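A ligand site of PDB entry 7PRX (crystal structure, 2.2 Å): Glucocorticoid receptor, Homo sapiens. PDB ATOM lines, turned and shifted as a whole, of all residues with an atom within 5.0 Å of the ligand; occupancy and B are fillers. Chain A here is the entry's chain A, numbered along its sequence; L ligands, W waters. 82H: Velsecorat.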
ATOM      1  N   GLU A  13      12.509 -19.413  13.534  1.00  0.00           N
ATOM      2  CA  GLU A  13      12.650 -18.435  12.443  1.00  0.00           C
ATOM      3  C   GLU A  13      12.281 -17.014  12.869  1.00  0.00           C
ATOM      4  O   GLU A  13      11.166 -16.794  13.342  1.00  0.00           O
ATOM      5  CB  GLU A  13      11.822 -18.840  11.218  1.00  0.00           C
ATOM      6  CG  GLU A  13      11.995 -17.889  10.034  1.00  0.00           C
ATOM      7  CD  GLU A  13      13.396 -17.732   9.461  1.00  0.00           C
ATOM      8  OE1 GLU A  13      13.659 -16.715   8.780  1.00  0.00           O
ATOM      9  OE2 GLU A  13      14.255 -18.607   9.742  1.00  0.00           O
ATOM     10  N   PRO A  14      13.234 -16.070  12.786  1.00  0.00           N
ATOM     11  CA  PRO A  14      12.950 -14.686  13.210  1.00  0.00           C
ATOM     12  C   PRO A  14      11.719 -14.073  12.562  1.00  0.00           C
ATOM     13  O   PRO A  14      11.477 -14.256  11.362  1.00  0.00           O
ATOM     14  CB  PRO A  14      14.192 -13.908  12.766  1.00  0.00           C
ATOM     15  CG  PRO A  14      15.260 -14.916  12.629  1.00  0.00           C
ATOM     16  CD  PRO A  14      14.610 -16.201  12.267  1.00  0.00           C
ATOM     17  N   ILE A  32      15.814   6.463   3.269  1.00  0.00           N
ATOM     18  CA  ILE A  32      15.617   5.018   3.081  1.00  0.00           C
ATOM     19  C   ILE A  32      16.816   4.184   3.541  1.00  0.00           C
ATOM     20  O   ILE A  32      16.653   3.167   4.203  1.00  0.00           O
ATOM     21  CB  ILE A  32      15.185   4.690   1.642  1.00  0.00           C
ATOM     22  CG1 ILE A  32      13.839   5.363   1.336  1.00  0.00           C
ATOM     23  CG2 ILE A  32      15.092   3.161   1.451  1.00  0.00           C
ATOM     24  CD1 ILE A  32      13.228   5.061  -0.064  1.00  0.00           C
ATOM     25  N   MET A  33      18.029   4.608   3.197  1.00  0.00           N
ATOM     26  CA  MET A  33      19.235   3.871   3.556  1.00  0.00           C
ATOM     27  C   MET A  33      19.524   3.958   5.029  1.00  0.00           C
ATOM     28  O   MET A  33      19.969   2.981   5.611  1.00  0.00           O
ATOM     29  CB  MET A  33      20.445   4.329   2.730  1.00  0.00           C
ATOM     30  CG  MET A  33      20.405   3.852   1.289  1.00  0.00           C
ATOM     31  SD  MET A  33      21.954   4.215   0.425  1.00  0.00           S
ATOM     32  CE  MET A  33      21.654   3.360  -1.138  1.00  0.00           C
ATOM     33  N   LEU A  36      16.889   1.654   6.618  1.00  0.00           N
ATOM     34  CA  LEU A  36      17.261   0.258   6.411  1.00  0.00           C
ATOM     35  C   LEU A  36      18.499  -0.115   7.208  1.00  0.00           C
ATOM     36  O   LEU A  36      18.600  -1.246   7.628  1.00  0.00           O
ATOM     37  CB  LEU A  36      17.404  -0.106   4.928  1.00  0.00           C
ATOM     38  CG  LEU A  36      16.085  -0.043   4.145  1.00  0.00           C
ATOM     39  CD1 LEU A  36      16.332  -0.275   2.629  1.00  0.00           C
ATOM     40  CD2 LEU A  36      15.070  -1.011   4.730  1.00  0.00           C
ATOM     41  N   ASN A  37      19.384   0.859   7.511  1.00  0.00           N
ATOM     42  CA  ASN A  37      20.530   0.603   8.358  1.00  0.00           C
ATOM     43  C   ASN A  37      20.073   0.303   9.788  1.00  0.00           C
ATOM     44  O   ASN A  37      20.462  -0.739  10.315  1.00  0.00           O
ATOM     45  CB  ASN A  37      21.537   1.749   8.321  1.00  0.00           C
ATOM     46  CG  ASN A  37      22.550   1.553   7.222  1.00  0.00           C
ATOM     47  OD1 ASN A  37      22.816   0.431   6.770  1.00  0.00           O
ATOM     48  ND2 ASN A  37      23.144   2.630   6.750  1.00  0.00           N
ATOM     49  N   LEU A  39      16.996  -0.601  10.856  1.00  0.00           N
ATOM     50  CA  LEU A  39      16.276  -1.877  10.748  1.00  0.00           C
ATOM     51  C   LEU A  39      17.301  -3.061  10.660  1.00  0.00           C
ATOM     52  O   LEU A  39      17.177  -4.039  11.405  1.00  0.00           O
ATOM     53  CB  LEU A  39      15.340  -1.887   9.508  1.00  0.00           C
ATOM     54  CG  LEU A  39      14.655  -3.247   9.223  1.00  0.00           C
ATOM     55  CD1 LEU A  39      13.868  -3.763  10.474  1.00  0.00           C
ATOM     56  CD2 LEU A  39      13.719  -3.154   8.040  1.00  0.00           C
ATOM     57  N   GLY A  40      18.338  -2.912   9.855  1.00  0.00           N
ATOM     58  CA  GLY A  40      19.391  -3.909   9.727  1.00  0.00           C
ATOM     59  C   GLY A  40      20.071  -4.312  11.022  1.00  0.00           C
ATOM     60  O   GLY A  40      20.343  -5.498  11.248  1.00  0.00           O
ATOM     61  N   GLN A  43      17.734  -6.542  12.775  1.00  0.00           N
ATOM     62  CA  GLN A  43      17.714  -7.854  12.117  1.00  0.00           C
ATOM     63  C   GLN A  43      18.964  -8.664  12.563  1.00  0.00           C
ATOM     64  O   GLN A  43      18.878  -9.878  12.830  1.00  0.00           O
ATOM     65  CB  GLN A  43      17.690  -7.697  10.581  1.00  0.00           C
ATOM     66  CG  GLN A  43      16.540  -6.815  10.032  1.00  0.00           C
ATOM     67  CD  GLN A  43      15.241  -7.567   9.787  1.00  0.00           C
ATOM     68  OE1 GLN A  43      14.953  -8.624  10.386  1.00  0.00           O
ATOM     69  NE2 GLN A  43      14.416  -7.039   8.908  1.00  0.00           N
ATOM     70  N   ALA A  46      18.096 -10.102  15.967  1.00  0.00           N
ATOM     71  CA  ALA A  46      17.250 -11.289  15.754  1.00  0.00           C
ATOM     72  C   ALA A  46      18.081 -12.479  15.282  1.00  0.00           C
ATOM     73  O   ALA A  46      17.807 -13.610  15.684  1.00  0.00           O
ATOM     74  CB  ALA A  46      16.171 -10.998  14.709  1.00  0.00           C
ATOM     75  N   ALA A  47      19.081 -12.239  14.423  1.00  0.00           N
ATOM     76  CA  ALA A  47      19.946 -13.319  13.919  1.00  0.00           C
ATOM     77  C   ALA A  47      20.786 -13.916  15.012  1.00  0.00           C
ATOM     78  O   ALA A  47      21.006 -15.127  14.987  1.00  0.00           O
ATOM     79  CB  ALA A  47      20.846 -12.804  12.803  1.00  0.00           C
ATOM     80  N   TRP A  73      26.579 -12.428   8.926  1.00  0.00           N
ATOM     81  CA  TRP A  73      25.430 -11.516   9.089  1.00  0.00           C
ATOM     82  C   TRP A  73      24.782 -11.039   7.758  1.00  0.00           C
ATOM     83  O   TRP A  73      23.560 -11.106   7.651  1.00  0.00           O
ATOM     84  CB  TRP A  73      25.780 -10.316  10.001  1.00  0.00           C
ATOM     85  CG  TRP A  73      26.726  -9.341   9.388  1.00  0.00           C
ATOM     86  CD1 TRP A  73      28.075  -9.468   9.261  1.00  0.00           C
ATOM     87  CD2 TRP A  73      26.372  -8.124   8.712  1.00  0.00           C
ATOM     88  NE1 TRP A  73      28.589  -8.405   8.548  1.00  0.00           N
ATOM     89  CE2 TRP A  73      27.561  -7.559   8.211  1.00  0.00           C
ATOM     90  CE3 TRP A  73      25.170  -7.431   8.520  1.00  0.00           C
ATOM     91  CZ2 TRP A  73      27.595  -6.321   7.572  1.00  0.00           C
ATOM     92  CZ3 TRP A  73      25.191  -6.237   7.824  1.00  0.00           C
ATOM     93  CH2 TRP A  73      26.399  -5.691   7.375  1.00  0.00           C
ATOM     94  N   MET A  74      25.561 -10.607   6.746  1.00  0.00           N
ATOM     95  CA  MET A  74      25.010 -10.122   5.471  1.00  0.00           C
ATOM     96  C   MET A  74      24.396 -11.246   4.627  1.00  0.00           C
ATOM     97  O   MET A  74      23.396 -11.048   3.944  1.00  0.00           O
ATOM     98  CB  MET A  74      26.046  -9.296   4.667  1.00  0.00           C
ATOM     99  CG  MET A  74      25.508  -8.662   3.369  1.00  0.00           C
ATOM    100  SD  MET A  74      24.012  -7.633   3.577  1.00  0.00           S
ATOM    101  CE  MET A  74      24.759  -6.071   4.144  1.00  0.00           C
ATOM    102  N   LEU A  76      22.795 -13.865   5.881  1.00  0.00           N
ATOM    103  CA  LEU A  76      21.475 -14.111   6.486  1.00  0.00           C
ATOM    104  C   LEU A  76      20.459 -13.041   6.061  1.00  0.00           C
ATOM    105  O   LEU A  76      19.370 -13.367   5.561  1.00  0.00           O
ATOM    106  CB  LEU A  76      21.602 -14.151   8.005  1.00  0.00           C
ATOM    107  CG  LEU A  76      22.578 -15.203   8.542  1.00  0.00           C
ATOM    108  CD1 LEU A  76      22.830 -14.980   9.976  1.00  0.00           C
ATOM    109  CD2 LEU A  76      22.052 -16.608   8.297  1.00  0.00           C
ATOM    110  N   MET A  77      20.822 -11.765   6.223  1.00  0.00           N
ATOM    111  CA  MET A  77      19.938 -10.678   5.853  1.00  0.00           C
ATOM    112  C   MET A  77      19.566 -10.704   4.377  1.00  0.00           C
ATOM    113  O   MET A  77      18.380 -10.651   4.055  1.00  0.00           O
ATOM    114  CB  MET A  77      20.553  -9.332   6.244  1.00  0.00           C
ATOM    115  CG  MET A  77      20.749  -9.203   7.763  1.00  0.00           C
ATOM    116  SD  MET A  77      20.456  -7.498   8.262  1.00  0.00           S
ATOM    117  CE  MET A  77      21.757  -6.649   7.277  1.00  0.00           C
ATOM    118  N   ALA A  78      20.547 -10.887   3.497  1.00  0.00           N
ATOM    119  CA  ALA A  78      20.299 -10.941   2.073  1.00  0.00           C
ATOM    120  C   ALA A  78      19.426 -12.110   1.708  1.00  0.00           C
ATOM    121  O   ALA A  78      18.530 -11.941   0.894  1.00  0.00           O
ATOM    122  CB  ALA A  78      21.604 -11.015   1.310  1.00  0.00           C
ATOM    123  N   ALA A  80      17.268 -13.915   3.665  1.00  0.00           N
ATOM    124  CA  ALA A  80      15.939 -13.787   4.240  1.00  0.00           C
ATOM    125  C   ALA A  80      15.159 -12.681   3.506  1.00  0.00           C
ATOM    126  O   ALA A  80      13.954 -12.796   3.327  1.00  0.00           O
ATOM    127  CB  ALA A  80      16.042 -13.522   5.717  1.00  0.00           C
ATOM    128  N   LEU A  81      15.843 -11.602   3.085  1.00  0.00           N
ATOM    129  CA  LEU A  81      15.222 -10.560   2.260  1.00  0.00           C
ATOM    130  C   LEU A  81      14.812 -11.184   0.913  1.00  0.00           C
ATOM    131  O   LEU A  81      13.710 -10.932   0.427  1.00  0.00           O
ATOM    132  CB  LEU A  81      16.217  -9.430   2.026  1.00  0.00           C
ATOM    133  CG  LEU A  81      15.789  -8.367   1.040  1.00  0.00           C
ATOM    134  CD1 LEU A  81      14.541  -7.606   1.510  1.00  0.00           C
ATOM    135  CD2 LEU A  81      16.914  -7.454   0.759  1.00  0.00           C
ATOM    136  N   CYS A  95      11.131  -6.544  -0.451  1.00  0.00           N
ATOM    137  CA  CYS A  95      10.240  -6.444   0.690  1.00  0.00           C
ATOM    138  C   CYS A  95      10.990  -6.399   1.991  1.00  0.00           C
ATOM    139  O   CYS A  95      10.942  -7.368   2.779  1.00  0.00           O
ATOM    140  CB  CYS A  95       9.224  -7.572   0.646  1.00  0.00           C
ATOM    141  SG  CYS A  95       8.280  -7.643  -0.906  1.00  0.00           S
ATOM    142  N   PHE A  96      11.698  -5.262   2.243  1.00  0.00           N
ATOM    143  CA  PHE A  96      12.499  -5.077   3.462  1.00  0.00           C
ATOM    144  C   PHE A  96      11.700  -5.234   4.738  1.00  0.00           C
ATOM    145  O   PHE A  96      12.015  -6.071   5.569  1.00  0.00           O
ATOM    146  CB  PHE A  96      13.235  -3.732   3.428  1.00  0.00           C
ATOM    147  CG  PHE A  96      14.448  -3.743   2.538  1.00  0.00           C
ATOM    148  CD1 PHE A  96      15.671  -4.190   3.025  1.00  0.00           C
ATOM    149  CD2 PHE A  96      14.363  -3.368   1.222  1.00  0.00           C
ATOM    150  CE1 PHE A  96      16.789  -4.243   2.185  1.00  0.00           C
ATOM    151  CE2 PHE A  96      15.495  -3.373   0.415  1.00  0.00           C
ATOM    152  CZ  PHE A  96      16.682  -3.841   0.892  1.00  0.00           C
ATOM    153  N   MET A 112      20.758   3.764  -5.013  1.00  0.00           N
ATOM    154  CA  MET A 112      19.898   2.635  -4.656  1.00  0.00           C
ATOM    155  C   MET A 112      20.059   1.348  -5.498  1.00  0.00           C
ATOM    156  O   MET A 112      20.281   0.283  -4.922  1.00  0.00           O
ATOM    157  CB  MET A 112      18.418   3.074  -4.682  1.00  0.00           C
ATOM    158  CG  MET A 112      18.014   3.904  -3.493  1.00  0.00           C
ATOM    159  SD  MET A 112      18.036   2.922  -1.988  1.00  0.00           S
ATOM    160  CE  MET A 112      16.752   1.762  -2.350  1.00  0.00           C
ATOM    161  N   GLN A 115      23.085  -1.676  -4.936  1.00  0.00           N
ATOM    162  CA  GLN A 115      22.902  -2.608  -3.832  1.00  0.00           C
ATOM    163  C   GLN A 115      21.639  -3.485  -4.028  1.00  0.00           C
ATOM    164  O   GLN A 115      21.649  -4.659  -3.658  1.00  0.00           O
ATOM    165  CB  GLN A 115      22.837  -1.830  -2.512  1.00  0.00           C
ATOM    166  CG  GLN A 115      23.254  -2.608  -1.280  1.00  0.00           C
ATOM    167  CD  GLN A 115      24.738  -2.867  -1.217  1.00  0.00           C
ATOM    168  OE1 GLN A 115      25.381  -3.183  -2.211  1.00  0.00           O
ATOM    169  NE2 GLN A 115      25.304  -2.759  -0.036  1.00  0.00           N
ATOM    170  N   CYS A 116      20.581  -2.887  -4.607  1.00  0.00           N
ATOM    171  CA  CYS A 116      19.301  -3.539  -4.894  1.00  0.00           C
ATOM    172  C   CYS A 116      19.430  -4.703  -5.885  1.00  0.00           C
ATOM    173  O   CYS A 116      18.937  -5.789  -5.595  1.00  0.00           O
ATOM    174  CB  CYS A 116      18.273  -2.516  -5.393  1.00  0.00           C
ATOM    175  SG  CYS A 116      17.471  -1.549  -4.089  1.00  0.00           S
ATOM    176  N   MET A 119      20.428  -7.922  -4.265  1.00  0.00           N
ATOM    177  CA  MET A 119      19.350  -8.420  -3.425  1.00  0.00           C
ATOM    178  C   MET A 119      18.276  -9.085  -4.294  1.00  0.00           C
ATOM    179  O   MET A 119      17.846 -10.192  -3.992  1.00  0.00           O
ATOM    180  CB  MET A 119      18.754  -7.272  -2.599  1.00  0.00           C
ATOM    181  CG  MET A 119      19.708  -6.762  -1.541  1.00  0.00           C
ATOM    182  SD  MET A 119      20.190  -8.055  -0.356  1.00  0.00           S
ATOM    183  CE  MET A 119      20.674  -7.041   1.026  1.00  0.00           C
ATOM    184  N   TYR A 136      14.636 -23.543   2.402  1.00  0.00           N
ATOM    185  CA  TYR A 136      15.058 -22.204   2.826  1.00  0.00           C
ATOM    186  C   TYR A 136      15.623 -22.188   4.266  1.00  0.00           C
ATOM    187  O   TYR A 136      16.636 -21.534   4.505  1.00  0.00           O
ATOM    188  CB  TYR A 136      13.893 -21.172   2.672  1.00  0.00           C
ATOM    189  CG  TYR A 136      14.029 -19.911   3.527  1.00  0.00           C
ATOM    190  CD1 TYR A 136      14.885 -18.881   3.170  1.00  0.00           C
ATOM    191  CD2 TYR A 136      13.301 -19.767   4.696  1.00  0.00           C
ATOM    192  CE1 TYR A 136      15.055 -17.759   3.977  1.00  0.00           C
ATOM    193  CE2 TYR A 136      13.449 -18.639   5.506  1.00  0.00           C
ATOM    194  CZ  TYR A 136      14.307 -17.623   5.123  1.00  0.00           C
ATOM    195  OH  TYR A 136      14.429 -16.484   5.900  1.00  0.00           O
ATOM    196  N   LYS A 140      19.472 -21.392   5.106  1.00  0.00           N
ATOM    197  CA  LYS A 140      19.819 -20.246   5.922  1.00  0.00           C
ATOM    198  C   LYS A 140      20.747 -20.617   7.087  1.00  0.00           C
ATOM    199  O   LYS A 140      21.734 -19.914   7.316  1.00  0.00           O
ATOM    200  CB  LYS A 140      18.571 -19.495   6.382  1.00  0.00           C
ATOM    201  CG  LYS A 140      18.912 -18.157   7.008  1.00  0.00           C
ATOM    202  CD  LYS A 140      17.805 -17.154   6.803  1.00  0.00           C
ATOM    203  CE  LYS A 140      16.969 -16.971   8.043  1.00  0.00           C
ATOM    204  NZ  LYS A 140      16.710 -18.229   8.770  1.00  0.00           N
ATOM    205  N   LEU A 205      27.715  -6.846  -1.793  1.00  0.00           N
ATOM    206  CA  LEU A 205      26.928  -6.125  -0.795  1.00  0.00           C
ATOM    207  C   LEU A 205      27.818  -5.427   0.230  1.00  0.00           C
ATOM    208  O   LEU A 205      27.662  -4.244   0.499  1.00  0.00           O
ATOM    209  CB  LEU A 205      25.944  -7.070  -0.101  1.00  0.00           C
ATOM    210  CG  LEU A 205      24.684  -7.434  -0.889  1.00  0.00           C
ATOM    211  CD1 LEU A 205      23.872  -8.475  -0.163  1.00  0.00           C
ATOM    212  CD2 LEU A 205      23.817  -6.220  -1.093  1.00  0.00           C
ATOM    213  N   TYR A 208      29.997  -2.347  -1.132  1.00  0.00           N
ATOM    214  CA  TYR A 208      29.259  -1.093  -1.203  1.00  0.00           C
ATOM    215  C   TYR A 208      28.975  -0.589   0.224  1.00  0.00           C
ATOM    216  O   TYR A 208      29.195   0.595   0.509  1.00  0.00           O
ATOM    217  CB  TYR A 208      27.980  -1.240  -2.033  1.00  0.00           C
ATOM    218  CG  TYR A 208      27.187   0.037  -2.128  1.00  0.00           C
ATOM    219  CD1 TYR A 208      27.518   1.025  -3.042  1.00  0.00           C
ATOM    220  CD2 TYR A 208      26.137   0.281  -1.251  1.00  0.00           C
ATOM    221  CE1 TYR A 208      26.805   2.223  -3.096  1.00  0.00           C
ATOM    222  CE2 TYR A 208      25.417   1.467  -1.303  1.00  0.00           C
ATOM    223  CZ  TYR A 208      25.755   2.440  -2.231  1.00  0.00           C
ATOM    224  OH  TYR A 208      25.047   3.615  -2.251  1.00  0.00           O
ATOM    225  N   CYS A 209      28.569  -1.504   1.132  1.00  0.00           N
ATOM    226  CA  CYS A 209      28.278  -1.243   2.546  1.00  0.00           C
ATOM    227  C   CYS A 209      29.470  -0.631   3.289  1.00  0.00           C
ATOM    228  O   CYS A 209      29.290   0.325   4.047  1.00  0.00           O
ATOM    229  CB  CYS A 209      27.787  -2.520   3.237  1.00  0.00           C
ATOM    230  SG  CYS A 209      27.601  -2.391   5.033  1.00  0.00           S
ATOM    231  N   THR A 212      30.097   2.944   2.116  1.00  0.00           N
ATOM    232  CA  THR A 212      29.109   3.855   2.710  1.00  0.00           C
ATOM    233  C   THR A 212      29.419   4.141   4.182  1.00  0.00           C
ATOM    234  O   THR A 212      29.216   5.266   4.642  1.00  0.00           O
ATOM    235  CB  THR A 212      27.693   3.297   2.517  1.00  0.00           C
ATOM    236  OG1 THR A 212      27.459   3.079   1.130  1.00  0.00           O
ATOM    237  CG2 THR A 212      26.630   4.213   3.054  1.00  0.00           C
ATOM    238  N   ILE A 220      25.304   8.883   5.838  1.00  0.00           N
ATOM    239  CA  ILE A 220      24.359   7.800   6.095  1.00  0.00           C
ATOM    240  C   ILE A 220      24.653   7.135   7.440  1.00  0.00           C
ATOM    241  O   ILE A 220      25.754   6.629   7.651  1.00  0.00           O
ATOM    242  CB  ILE A 220      24.355   6.816   4.905  1.00  0.00           C
ATOM    243  CG1 ILE A 220      23.707   7.471   3.675  1.00  0.00           C
ATOM    244  CG2 ILE A 220      23.647   5.521   5.254  1.00  0.00           C
ATOM    245  CD1 ILE A 220      24.216   6.964   2.277  1.00  0.00           C
ATOM    246  N   PHE A 222      24.505   4.538  10.797  1.00  0.00           N
ATOM    247  CA  PHE A 222      24.527   3.108  11.045  1.00  0.00           C
ATOM    248  C   PHE A 222      24.184   2.832  12.494  1.00  0.00           C
ATOM    249  O   PHE A 222      24.599   3.584  13.394  1.00  0.00           O
ATOM    250  CB  PHE A 222      25.915   2.516  10.708  1.00  0.00           C
ATOM    251  CG  PHE A 222      26.146   2.284   9.233  1.00  0.00           C
ATOM    252  CD1 PHE A 222      26.566   3.314   8.410  1.00  0.00           C
ATOM    253  CD2 PHE A 222      25.918   1.044   8.670  1.00  0.00           C
ATOM    254  CE1 PHE A 222      26.770   3.100   7.048  1.00  0.00           C
ATOM    255  CE2 PHE A 222      26.150   0.822   7.317  1.00  0.00           C
ATOM    256  CZ  PHE A 222      26.568   1.848   6.518  1.00  0.00           C
ATOM    257  N   LEU A 226      25.716  -2.712  13.926  1.00  0.00           N
ATOM    258  CA  LEU A 226      26.375  -2.810  12.616  1.00  0.00           C
ATOM    259  C   LEU A 226      27.681  -2.050  12.578  1.00  0.00           C
ATOM    260  O   LEU A 226      28.634  -2.512  11.955  1.00  0.00           O
ATOM    261  CB  LEU A 226      25.462  -2.344  11.475  1.00  0.00           C
ATOM    262  CG  LEU A 226      24.206  -3.175  11.170  1.00  0.00           C
ATOM    263  CD1 LEU A 226      23.662  -2.828   9.803  1.00  0.00           C
ATOM    264  CD2 LEU A 226      24.488  -4.648  11.174  1.00  0.00           C
HETATM  265  C1  82H L   1      14.348  -8.787   5.454  1.00  0.00           C
HETATM  266  C2  82H L   1      14.900  -9.730   6.300  1.00  0.00           C
HETATM  267  C3  82H L   1      20.658  -0.649   3.560  1.00  0.00           C
HETATM  268  C7  82H L   1      19.942  -5.735   4.351  1.00  0.00           C
HETATM  269  C8  82H L   1      19.414  -3.879   5.799  1.00  0.00           C
HETATM  270  C9  82H L   1      16.710  -8.251   6.830  1.00  0.00           C
HETATM  271  C10 82H L   1      20.806  -2.626   2.271  1.00  0.00           C
HETATM  272  C11 82H L   1      17.066  -4.172   6.819  1.00  0.00           C
HETATM  273  C12 82H L   1      18.207  -4.509   6.041  1.00  0.00           C
HETATM  274  C13 82H L   1      16.078  -9.468   6.968  1.00  0.00           C
HETATM  275  C14 82H L   1      21.042  -1.968   3.457  1.00  0.00           C
HETATM  276  C15 82H L   1      17.904  -5.707   5.442  1.00  0.00           C
HETATM  277  C16 82H L   1      16.135  -7.326   5.993  1.00  0.00           C
HETATM  278  C19 82H L   1      20.260  -4.540   4.933  1.00  0.00           C
HETATM  279  C20 82H L   1      16.624 -10.468   7.911  1.00  0.00           C
HETATM  280  C21 82H L   1      24.126  -0.753   3.289  1.00  0.00           C
HETATM  281  C22 82H L   1      16.422 -11.673  10.772  1.00  0.00           C
HETATM  282  C24 82H L   1      19.346  -0.591  -0.963  1.00  0.00           C
HETATM  283  C27 82H L   1      15.765 -12.256   9.541  1.00  0.00           C
HETATM  284  C30 82H L   1      21.670  -2.651   4.644  1.00  0.00           C
HETATM  285  C31 82H L   1      23.146  -2.427   4.727  1.00  0.00           C
HETATM  286  C32 82H L   1      24.483   0.682   3.104  1.00  0.00           C
HETATM  287  C4  82H L   1      18.749  -6.383   4.591  1.00  0.00           C
HETATM  288  C5  82H L   1      14.972  -7.574   5.311  1.00  0.00           C
HETATM  289  C6  82H L   1      20.073   0.022   2.518  1.00  0.00           C
HETATM  290  C17 82H L   1      19.865  -0.637   1.334  1.00  0.00           C
HETATM  291  C18 82H L   1      20.206  -1.972   1.226  1.00  0.00           C
HETATM  292  C23 82H L   1      17.683 -12.486  10.977  1.00  0.00           C
HETATM  293  C25 82H L   1      18.994  -2.052  -0.760  1.00  0.00           C
HETATM  294  C26 82H L   1      16.483 -13.549   9.295  1.00  0.00           C
HETATM  295  C28 82H L   1      23.667  -2.894   6.045  1.00  0.00           C
HETATM  296  C29 82H L   1      23.501   1.205   2.096  1.00  0.00           C
HETATM  297  N33 82H L   1      16.116  -5.109   6.701  1.00  0.00           N
HETATM  298  N34 82H L   1      16.660  -6.042   5.897  1.00  0.00           N
HETATM  299  N35 82H L   1      15.709 -11.422   8.351  1.00  0.00           N
HETATM  300  N36 82H L   1      23.538  -1.073   4.494  1.00  0.00           N
HETATM  301  O37 82H L   1      17.771 -10.298   8.307  1.00  0.00           O
HETATM  302  O38 82H L   1      24.325  -1.558   2.386  1.00  0.00           O
HETATM  303  O39 82H L   1      19.252   0.087   0.298  1.00  0.00           O
HETATM  304  O40 82H L   1      20.011  -2.672   0.044  1.00  0.00           O
HETATM  305  O41 82H L   1      17.699 -13.555  10.028  1.00  0.00           O
HETATM  306  O42 82H L   1      21.524  -4.072   4.595  1.00  0.00           O
HETATM  307  F43 82H L   1      24.482   1.416   4.247  1.00  0.00           F
HETATM  308  F44 82H L   1      25.732   0.845   2.594  1.00  0.00           F
HETATM  309  O   HOH W   1      18.854 -15.849  10.074  1.00  0.00           O
HETATM  310  O   HOH W   2      12.912 -11.983   8.143  1.00  0.00           O
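Water W1 lies within hydrogen-bond range of O41 of the ligand and NZ of Lys 140.
The side-chain amide nitrogen of Asn 37 sits close to the backbone carbonyl oxygen of Met 33, at 3.4 Å. The side-chain amide nitrogen of Gln 115 sits at hydrogen-bond distance from the backbone carbonyl oxygen of Leu 205 (2.8 Å). OG1 of Thr 212 sits at hydrogen-bond distance from O of Tyr 208 (3.1 Å). The side-chain carboxylate of Glu 13 lies within salt-bridge range of the side-chain amino group of Lys 140 (2.7 Å). SG of Cys 116 is in hydrogen-bond range of O of Met 112.
OD1 of Asn 37 is in hydrogen-bond range of N36 of the ligand (2.8 Å). An oxygen (O38) of the ligand is in hydrogen-bond range of the side-chain amide nitrogen of Gln 115 (2.9 Å). N33 of the ligand lies close to NE2 of Gln 43.
The side-chain hydroxyl of Thr 212 lies close to a fluorine (F44) of the ligand (3.2 Å). Pro 14 touches the ligand (CB to C22, 3.7 Å). Met 33 touches the ligand. Leu 36 touches the ligand (O to C8, 3.3 Å). CD2 of Leu 39 touches N33 of the ligand, at 3.4 Å. Gly 40 touches the ligand. Ala 47 touches the ligand. Met 74 touches the ligand. Met 77 touches the ligand. Ala 80 touches the ligand. Leu 81 touches the ligand (CA to C1, 3.8 Å). Phe 96 touches the ligand. Met 112 touches the ligand. SG of Cys 116 touches C25 of the ligand (3.7 Å). CE of Met 119 touches C7 of the ligand, 3.6 Å away. Lys 140 touches the ligand. Tyr 208 touches the ligand (CD2 to F44, 3.9 Å). Cys 209 touches the ligand (CA to F44, 3.3 Å). Phe 222 touches the ligand. Leu 226 touches the ligand. Hydrophobic or aromatic side chains that line the ligand: Pro 14, Met 33, Leu 36, Leu 39, Ala 47, Met 74, Met 77, Ala 80, Leu 81, Phe 96, Met 112, Met 119, Tyr 208, Phe 222 and Leu 226. Of the 33 residues printed, 23 come within 4 Å of the ligand.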
